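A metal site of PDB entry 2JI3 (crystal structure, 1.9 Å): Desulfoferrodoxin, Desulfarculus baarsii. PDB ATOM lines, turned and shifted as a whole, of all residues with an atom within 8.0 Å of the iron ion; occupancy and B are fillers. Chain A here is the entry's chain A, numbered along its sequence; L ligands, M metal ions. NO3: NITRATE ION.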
ATOM      1  N   VAL A  42     -11.221 -29.076  18.691  1.00  0.00           N
ATOM      2  CA  VAL A  42     -11.601 -30.242  17.894  1.00  0.00           C
ATOM      3  C   VAL A  42     -10.654 -30.443  16.707  1.00  0.00           C
ATOM      4  O   VAL A  42     -10.207 -29.491  16.075  1.00  0.00           O
ATOM      5  CB  VAL A  42     -13.062 -30.109  17.369  1.00  0.00           C
ATOM      6  CG1 VAL A  42     -13.366 -31.207  16.365  1.00  0.00           C
ATOM      7  CG2 VAL A  42     -14.036 -30.186  18.538  1.00  0.00           C
ATOM      8  N   ALA A  44     -10.195 -30.822  13.380  1.00  0.00           N
ATOM      9  CA  ALA A  44     -10.865 -30.624  12.099  1.00  0.00           C
ATOM     10  C   ALA A  44     -10.117 -29.592  11.258  1.00  0.00           C
ATOM     11  O   ALA A  44      -9.220 -28.914  11.746  1.00  0.00           O
ATOM     12  CB  ALA A  44     -12.308 -30.185  12.324  1.00  0.00           C
ATOM     13  N   ALA A  45     -10.513 -29.474   9.992  1.00  0.00           N
ATOM     14  CA  ALA A  45      -9.895 -28.549   9.049  1.00  0.00           C
ATOM     15  C   ALA A  45     -10.065 -27.100   9.502  1.00  0.00           C
ATOM     16  O   ALA A  45     -11.155 -26.533   9.394  1.00  0.00           O
ATOM     17  CB  ALA A  45     -10.499 -28.729   7.663  1.00  0.00           C
ATOM     18  N   LYS A  48     -11.697 -24.501   7.308  1.00  0.00           N
ATOM     19  CA  LYS A  48     -13.139 -24.584   7.131  1.00  0.00           C
ATOM     20  C   LYS A  48     -13.923 -24.176   8.381  1.00  0.00           C
ATOM     21  O   LYS A  48     -15.136 -23.967   8.296  1.00  0.00           O
ATOM     22  CB  LYS A  48     -13.546 -26.011   6.738  1.00  0.00           C
ATOM     23  CG  LYS A  48     -13.056 -26.452   5.373  1.00  0.00           C
ATOM     24  CD  LYS A  48     -13.583 -27.831   5.033  1.00  0.00           C
ATOM     25  CE  LYS A  48     -13.148 -28.281   3.658  1.00  0.00           C
ATOM     26  NZ  LYS A  48     -13.732 -29.628   3.354  1.00  0.00           N
ATOM     27  N   HIS A  49     -13.239 -24.063   9.519  1.00  0.00           N
ATOM     28  CA  HIS A  49     -13.920 -23.715  10.777  1.00  0.00           C
ATOM     29  C   HIS A  49     -13.538 -22.416  11.478  1.00  0.00           C
ATOM     30  O   HIS A  49     -14.395 -21.774  12.089  1.00  0.00           O
ATOM     31  CB  HIS A  49     -13.790 -24.872  11.775  1.00  0.00           C
ATOM     32  CG  HIS A  49     -14.422 -26.151  11.305  1.00  0.00           C
ATOM     33  ND1 HIS A  49     -13.742 -27.099  10.565  1.00  0.00           N
ATOM     34  CD2 HIS A  49     -15.679 -26.611  11.448  1.00  0.00           C
ATOM     35  CE1 HIS A  49     -14.560 -28.096  10.275  1.00  0.00           C
ATOM     36  NE2 HIS A  49     -15.748 -27.827  10.792  1.00  0.00           N
ATOM     37  N   VAL A  64     -17.048 -18.327   7.657  1.00  0.00           N
ATOM     38  CA  VAL A  64     -16.538 -19.564   8.172  1.00  0.00           C
ATOM     39  C   VAL A  64     -16.250 -20.651   7.112  1.00  0.00           C
ATOM     40  O   VAL A  64     -17.195 -21.277   6.629  1.00  0.00           O
ATOM     41  CB  VAL A  64     -17.604 -20.172   9.168  1.00  0.00           C
ATOM     42  CG1 VAL A  64     -17.098 -21.474   9.728  1.00  0.00           C
ATOM     43  CG2 VAL A  64     -17.914 -19.145  10.248  1.00  0.00           C
ATOM     44  N   HIS A  69     -17.304 -23.227   4.527  1.00  0.00           N
ATOM     45  CA  HIS A  69     -17.656 -24.470   5.210  1.00  0.00           C
ATOM     46  C   HIS A  69     -18.966 -24.996   4.631  1.00  0.00           C
ATOM     47  O   HIS A  69     -19.812 -24.225   4.180  1.00  0.00           O
ATOM     48  CB  HIS A  69     -17.802 -24.221   6.719  1.00  0.00           C
ATOM     49  CG  HIS A  69     -18.140 -25.452   7.508  1.00  0.00           C
ATOM     50  ND1 HIS A  69     -19.381 -26.051   7.461  1.00  0.00           N
ATOM     51  CD2 HIS A  69     -17.398 -26.182   8.366  1.00  0.00           C
ATOM     52  CE1 HIS A  69     -19.380 -27.104   8.260  1.00  0.00           C
ATOM     53  NE2 HIS A  69     -18.193 -27.209   8.818  1.00  0.00           N
ATOM     54  N   PRO A  70     -19.147 -26.325   4.621  1.00  0.00           N
ATOM     55  CA  PRO A  70     -20.386 -26.896   4.096  1.00  0.00           C
ATOM     56  C   PRO A  70     -21.610 -26.419   4.887  1.00  0.00           C
ATOM     57  O   PRO A  70     -21.509 -26.138   6.087  1.00  0.00           O
ATOM     58  CB  PRO A  70     -20.178 -28.395   4.241  1.00  0.00           C
ATOM     59  CG  PRO A  70     -18.696 -28.543   4.110  1.00  0.00           C
ATOM     60  CD  PRO A  70     -18.164 -27.385   4.926  1.00  0.00           C
ATOM     61  N   LYS A  74     -26.927 -32.363   7.347  1.00  0.00           N
ATOM     62  CA  LYS A  74     -26.239 -33.129   8.374  1.00  0.00           C
ATOM     63  C   LYS A  74     -24.899 -32.523   8.789  1.00  0.00           C
ATOM     64  O   LYS A  74     -24.233 -33.030   9.680  1.00  0.00           O
ATOM     65  CB  LYS A  74     -26.026 -34.577   7.922  1.00  0.00           C
ATOM     66  CG  LYS A  74     -27.321 -35.372   7.728  1.00  0.00           C
ATOM     67  CD  LYS A  74     -27.038 -36.859   7.534  1.00  0.00           C
ATOM     68  CE  LYS A  74     -28.320 -37.671   7.445  1.00  0.00           C
ATOM     69  NZ  LYS A  74     -28.076 -39.151   7.414  1.00  0.00           N
ATOM     70  N   HIS A  75     -24.512 -31.434   8.149  1.00  0.00           N
ATOM     71  CA  HIS A  75     -23.240 -30.795   8.466  1.00  0.00           C
ATOM     72  C   HIS A  75     -23.267 -29.318   8.068  1.00  0.00           C
ATOM     73  O   HIS A  75     -23.085 -28.978   6.897  1.00  0.00           O
ATOM     74  CB  HIS A  75     -22.124 -31.513   7.708  1.00  0.00           C
ATOM     75  CG  HIS A  75     -20.755 -31.017   8.037  1.00  0.00           C
ATOM     76  ND1 HIS A  75     -19.699 -31.094   7.168  1.00  0.00           N
ATOM     77  CD2 HIS A  75     -20.271 -30.445   9.171  1.00  0.00           C
ATOM     78  CE1 HIS A  75     -18.622 -30.595   7.731  1.00  0.00           C
ATOM     79  NE2 HIS A  75     -18.933 -30.190   8.953  1.00  0.00           N
ATOM     80  N   TYR A  76     -23.509 -28.439   9.040  1.00  0.00           N
ATOM     81  CA  TYR A  76     -23.542 -27.014   8.731  1.00  0.00           C
ATOM     82  C   TYR A  76     -23.158 -26.158   9.931  1.00  0.00           C
ATOM     83  O   TYR A  76     -23.077 -26.647  11.052  1.00  0.00           O
ATOM     84  CB  TYR A  76     -24.954 -26.605   8.261  1.00  0.00           C
ATOM     85  CG  TYR A  76     -26.037 -26.703   9.327  1.00  0.00           C
ATOM     86  CD1 TYR A  76     -26.504 -27.949   9.760  1.00  0.00           C
ATOM     87  CD2 TYR A  76     -26.597 -25.556   9.896  1.00  0.00           C
ATOM     88  CE1 TYR A  76     -27.506 -28.042  10.737  1.00  0.00           C
ATOM     89  CE2 TYR A  76     -27.592 -25.642  10.869  1.00  0.00           C
ATOM     90  CZ  TYR A  76     -28.040 -26.889  11.281  1.00  0.00           C
ATOM     91  OH  TYR A  76     -29.044 -26.980  12.228  1.00  0.00           O
ATOM     92  N   ILE A  77     -22.920 -24.878   9.682  1.00  0.00           N
ATOM     93  CA  ILE A  77     -22.584 -23.927  10.735  1.00  0.00           C
ATOM     94  C   ILE A  77     -23.932 -23.453  11.286  1.00  0.00           C
ATOM     95  O   ILE A  77     -24.702 -22.799  10.575  1.00  0.00           O
ATOM     96  CB  ILE A  77     -21.806 -22.715  10.189  1.00  0.00           C
ATOM     97  CG1 ILE A  77     -20.494 -23.185   9.550  1.00  0.00           C
ATOM     98  CG2 ILE A  77     -21.547 -21.715  11.296  1.00  0.00           C
ATOM     99  CD1 ILE A  77     -19.662 -24.095  10.452  1.00  0.00           C
ATOM    100  N   TYR A 115     -20.101 -22.150  15.275  1.00  0.00           N
ATOM    101  CA  TYR A 115     -20.328 -23.492  15.769  1.00  0.00           C
ATOM    102  C   TYR A 115     -20.801 -24.447  14.672  1.00  0.00           C
ATOM    103  O   TYR A 115     -21.836 -24.218  14.037  1.00  0.00           O
ATOM    104  CB  TYR A 115     -21.356 -23.481  16.909  1.00  0.00           C
ATOM    105  CG  TYR A 115     -21.534 -24.835  17.586  1.00  0.00           C
ATOM    106  CD1 TYR A 115     -22.483 -25.752  17.133  1.00  0.00           C
ATOM    107  CD2 TYR A 115     -20.709 -25.215  18.641  1.00  0.00           C
ATOM    108  CE1 TYR A 115     -22.609 -27.022  17.723  1.00  0.00           C
ATOM    109  CE2 TYR A 115     -20.817 -26.469  19.236  1.00  0.00           C
ATOM    110  CZ  TYR A 115     -21.769 -27.370  18.781  1.00  0.00           C
ATOM    111  OH  TYR A 115     -21.875 -28.605  19.388  1.00  0.00           O
ATOM    112  N   CYS A 116     -20.054 -25.519  14.481  1.00  0.00           N
ATOM    113  CA  CYS A 116     -20.382 -26.535  13.492  1.00  0.00           C
ATOM    114  C   CYS A 116     -21.094 -27.651  14.253  1.00  0.00           C
ATOM    115  O   CYS A 116     -20.598 -28.085  15.285  1.00  0.00           O
ATOM    116  CB  CYS A 116     -19.101 -27.080  12.855  1.00  0.00           C
ATOM    117  SG  CYS A 116     -19.364 -28.495  11.781  1.00  0.00           S
ATOM    118  N   ASN A 117     -22.238 -28.111  13.743  1.00  0.00           N
ATOM    119  CA  ASN A 117     -22.978 -29.158  14.432  1.00  0.00           C
ATOM    120  C   ASN A 117     -22.150 -30.424  14.633  1.00  0.00           C
ATOM    121  O   ASN A 117     -22.395 -31.187  15.570  1.00  0.00           O
ATOM    122  CB  ASN A 117     -24.288 -29.489  13.700  1.00  0.00           C
ATOM    123  CG  ASN A 117     -24.075 -30.208  12.370  1.00  0.00           C
ATOM    124  OD1 ASN A 117     -23.300 -29.759  11.518  1.00  0.00           O
ATOM    125  ND2 ASN A 117     -24.782 -31.314  12.179  1.00  0.00           N
ATOM    126  N   ILE A 118     -21.160 -30.628  13.774  1.00  0.00           N
ATOM    127  CA  ILE A 118     -20.303 -31.803  13.887  1.00  0.00           C
ATOM    128  C   ILE A 118     -18.946 -31.490  14.538  1.00  0.00           C
ATOM    129  O   ILE A 118     -18.572 -32.122  15.514  1.00  0.00           O
ATOM    130  CB  ILE A 118     -20.043 -32.447  12.503  1.00  0.00           C
ATOM    131  CG1 ILE A 118     -21.369 -32.835  11.834  1.00  0.00           C
ATOM    132  CG2 ILE A 118     -19.138 -33.660  12.668  1.00  0.00           C
ATOM    133  CD1 ILE A 118     -22.227 -33.773  12.661  1.00  0.00           C
ATOM    134  N   HIS A 119     -18.246 -30.501  14.004  1.00  0.00           N
ATOM    135  CA  HIS A 119     -16.908 -30.162  14.497  1.00  0.00           C
ATOM    136  C   HIS A 119     -16.737 -29.178  15.659  1.00  0.00           C
ATOM    137  O   HIS A 119     -15.621 -28.744  15.957  1.00  0.00           O
ATOM    138  CB  HIS A 119     -16.060 -29.730  13.305  1.00  0.00           C
ATOM    139  CG  HIS A 119     -16.038 -30.756  12.208  1.00  0.00           C
ATOM    140  ND1 HIS A 119     -16.654 -30.564  10.993  1.00  0.00           N
ATOM    141  CD2 HIS A 119     -15.544 -32.023  12.195  1.00  0.00           C
ATOM    142  CE1 HIS A 119     -16.548 -31.673  10.272  1.00  0.00           C
ATOM    143  NE2 HIS A 119     -15.879 -32.568  10.975  1.00  0.00           N
ATOM    144  N   GLY A 120     -17.829 -28.809  16.314  1.00  0.00           N
ATOM    145  CA  GLY A 120     -17.724 -27.931  17.467  1.00  0.00           C
ATOM    146  C   GLY A 120     -17.569 -26.424  17.358  1.00  0.00           C
ATOM    147  O   GLY A 120     -17.894 -25.793  16.358  1.00  0.00           O
ATOM    148  N   TRP A 122     -15.517 -22.780  17.462  1.00  0.00           N
ATOM    149  CA  TRP A 122     -14.282 -22.180  16.942  1.00  0.00           C
ATOM    150  C   TRP A 122     -14.317 -20.665  17.070  1.00  0.00           C
ATOM    151  O   TRP A 122     -15.396 -20.063  17.103  1.00  0.00           O
ATOM    152  CB  TRP A 122     -14.083 -22.557  15.471  1.00  0.00           C
ATOM    153  CG  TRP A 122     -13.947 -24.032  15.271  1.00  0.00           C
ATOM    154  CD1 TRP A 122     -14.935 -24.966  15.329  1.00  0.00           C
ATOM    155  CD2 TRP A 122     -12.722 -24.764  15.086  1.00  0.00           C
ATOM    156  NE1 TRP A 122     -14.414 -26.228  15.207  1.00  0.00           N
ATOM    157  CE2 TRP A 122     -13.060 -26.137  15.062  1.00  0.00           C
ATOM    158  CE3 TRP A 122     -11.379 -24.389  14.955  1.00  0.00           C
ATOM    159  CZ2 TRP A 122     -12.089 -27.136  14.895  1.00  0.00           C
ATOM    160  CZ3 TRP A 122     -10.417 -25.388  14.799  1.00  0.00           C
ATOM    161  CH2 TRP A 122     -10.788 -26.742  14.774  1.00  0.00           C
HETATM  162  N   NO3 L   1     -15.347 -29.957   6.961  1.00  0.00           N
HETATM  163  O1  NO3 L   1     -15.824 -29.859   5.840  1.00  0.00           O
HETATM  164  O2  NO3 L   1     -14.305 -30.563   7.131  1.00  0.00           O
HETATM  165  O3  NO3 L   1     -15.915 -29.443   7.920  1.00  0.00           O
HETATM  166 FE    FE M   1     -17.534 -28.956  10.101  1.00  0.00          FE
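The backbone carbonyl oxygen of His 119 lies within hydrogen-bond range of the indole nitrogen of Trp 122.
A ring nitrogen (ND1) of His 49 sits at hydrogen-bond distance from the backbone carbonyl oxygen (O) of Ala 45 (2.9 Å).
The backbone carbonyl oxygen of Val 64 sits at hydrogen-bond distance from the backbone NH of His 69 (2.9 Å).
The side-chain sulfur (SG) of Cys 116 sits close to the backbone NH (N) of Ile 118 (3.4 Å).
ND1 of His 119 binds the iron ion.
A ring nitrogen (NE2) of His 75 is bound to the iron ion, at 2.2 Å.
A ring nitrogen (NE2) of His 49 binds the iron ion (2.2 Å).
The iron ion is bound by NE2 of His 69 (2.3 Å).
The side-chain sulfur (SG) of Cys 116 is bound to the iron ion (2.5 Å).
Slightly farther from the iron ion lies O3 of the ligand (2.8 Å).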
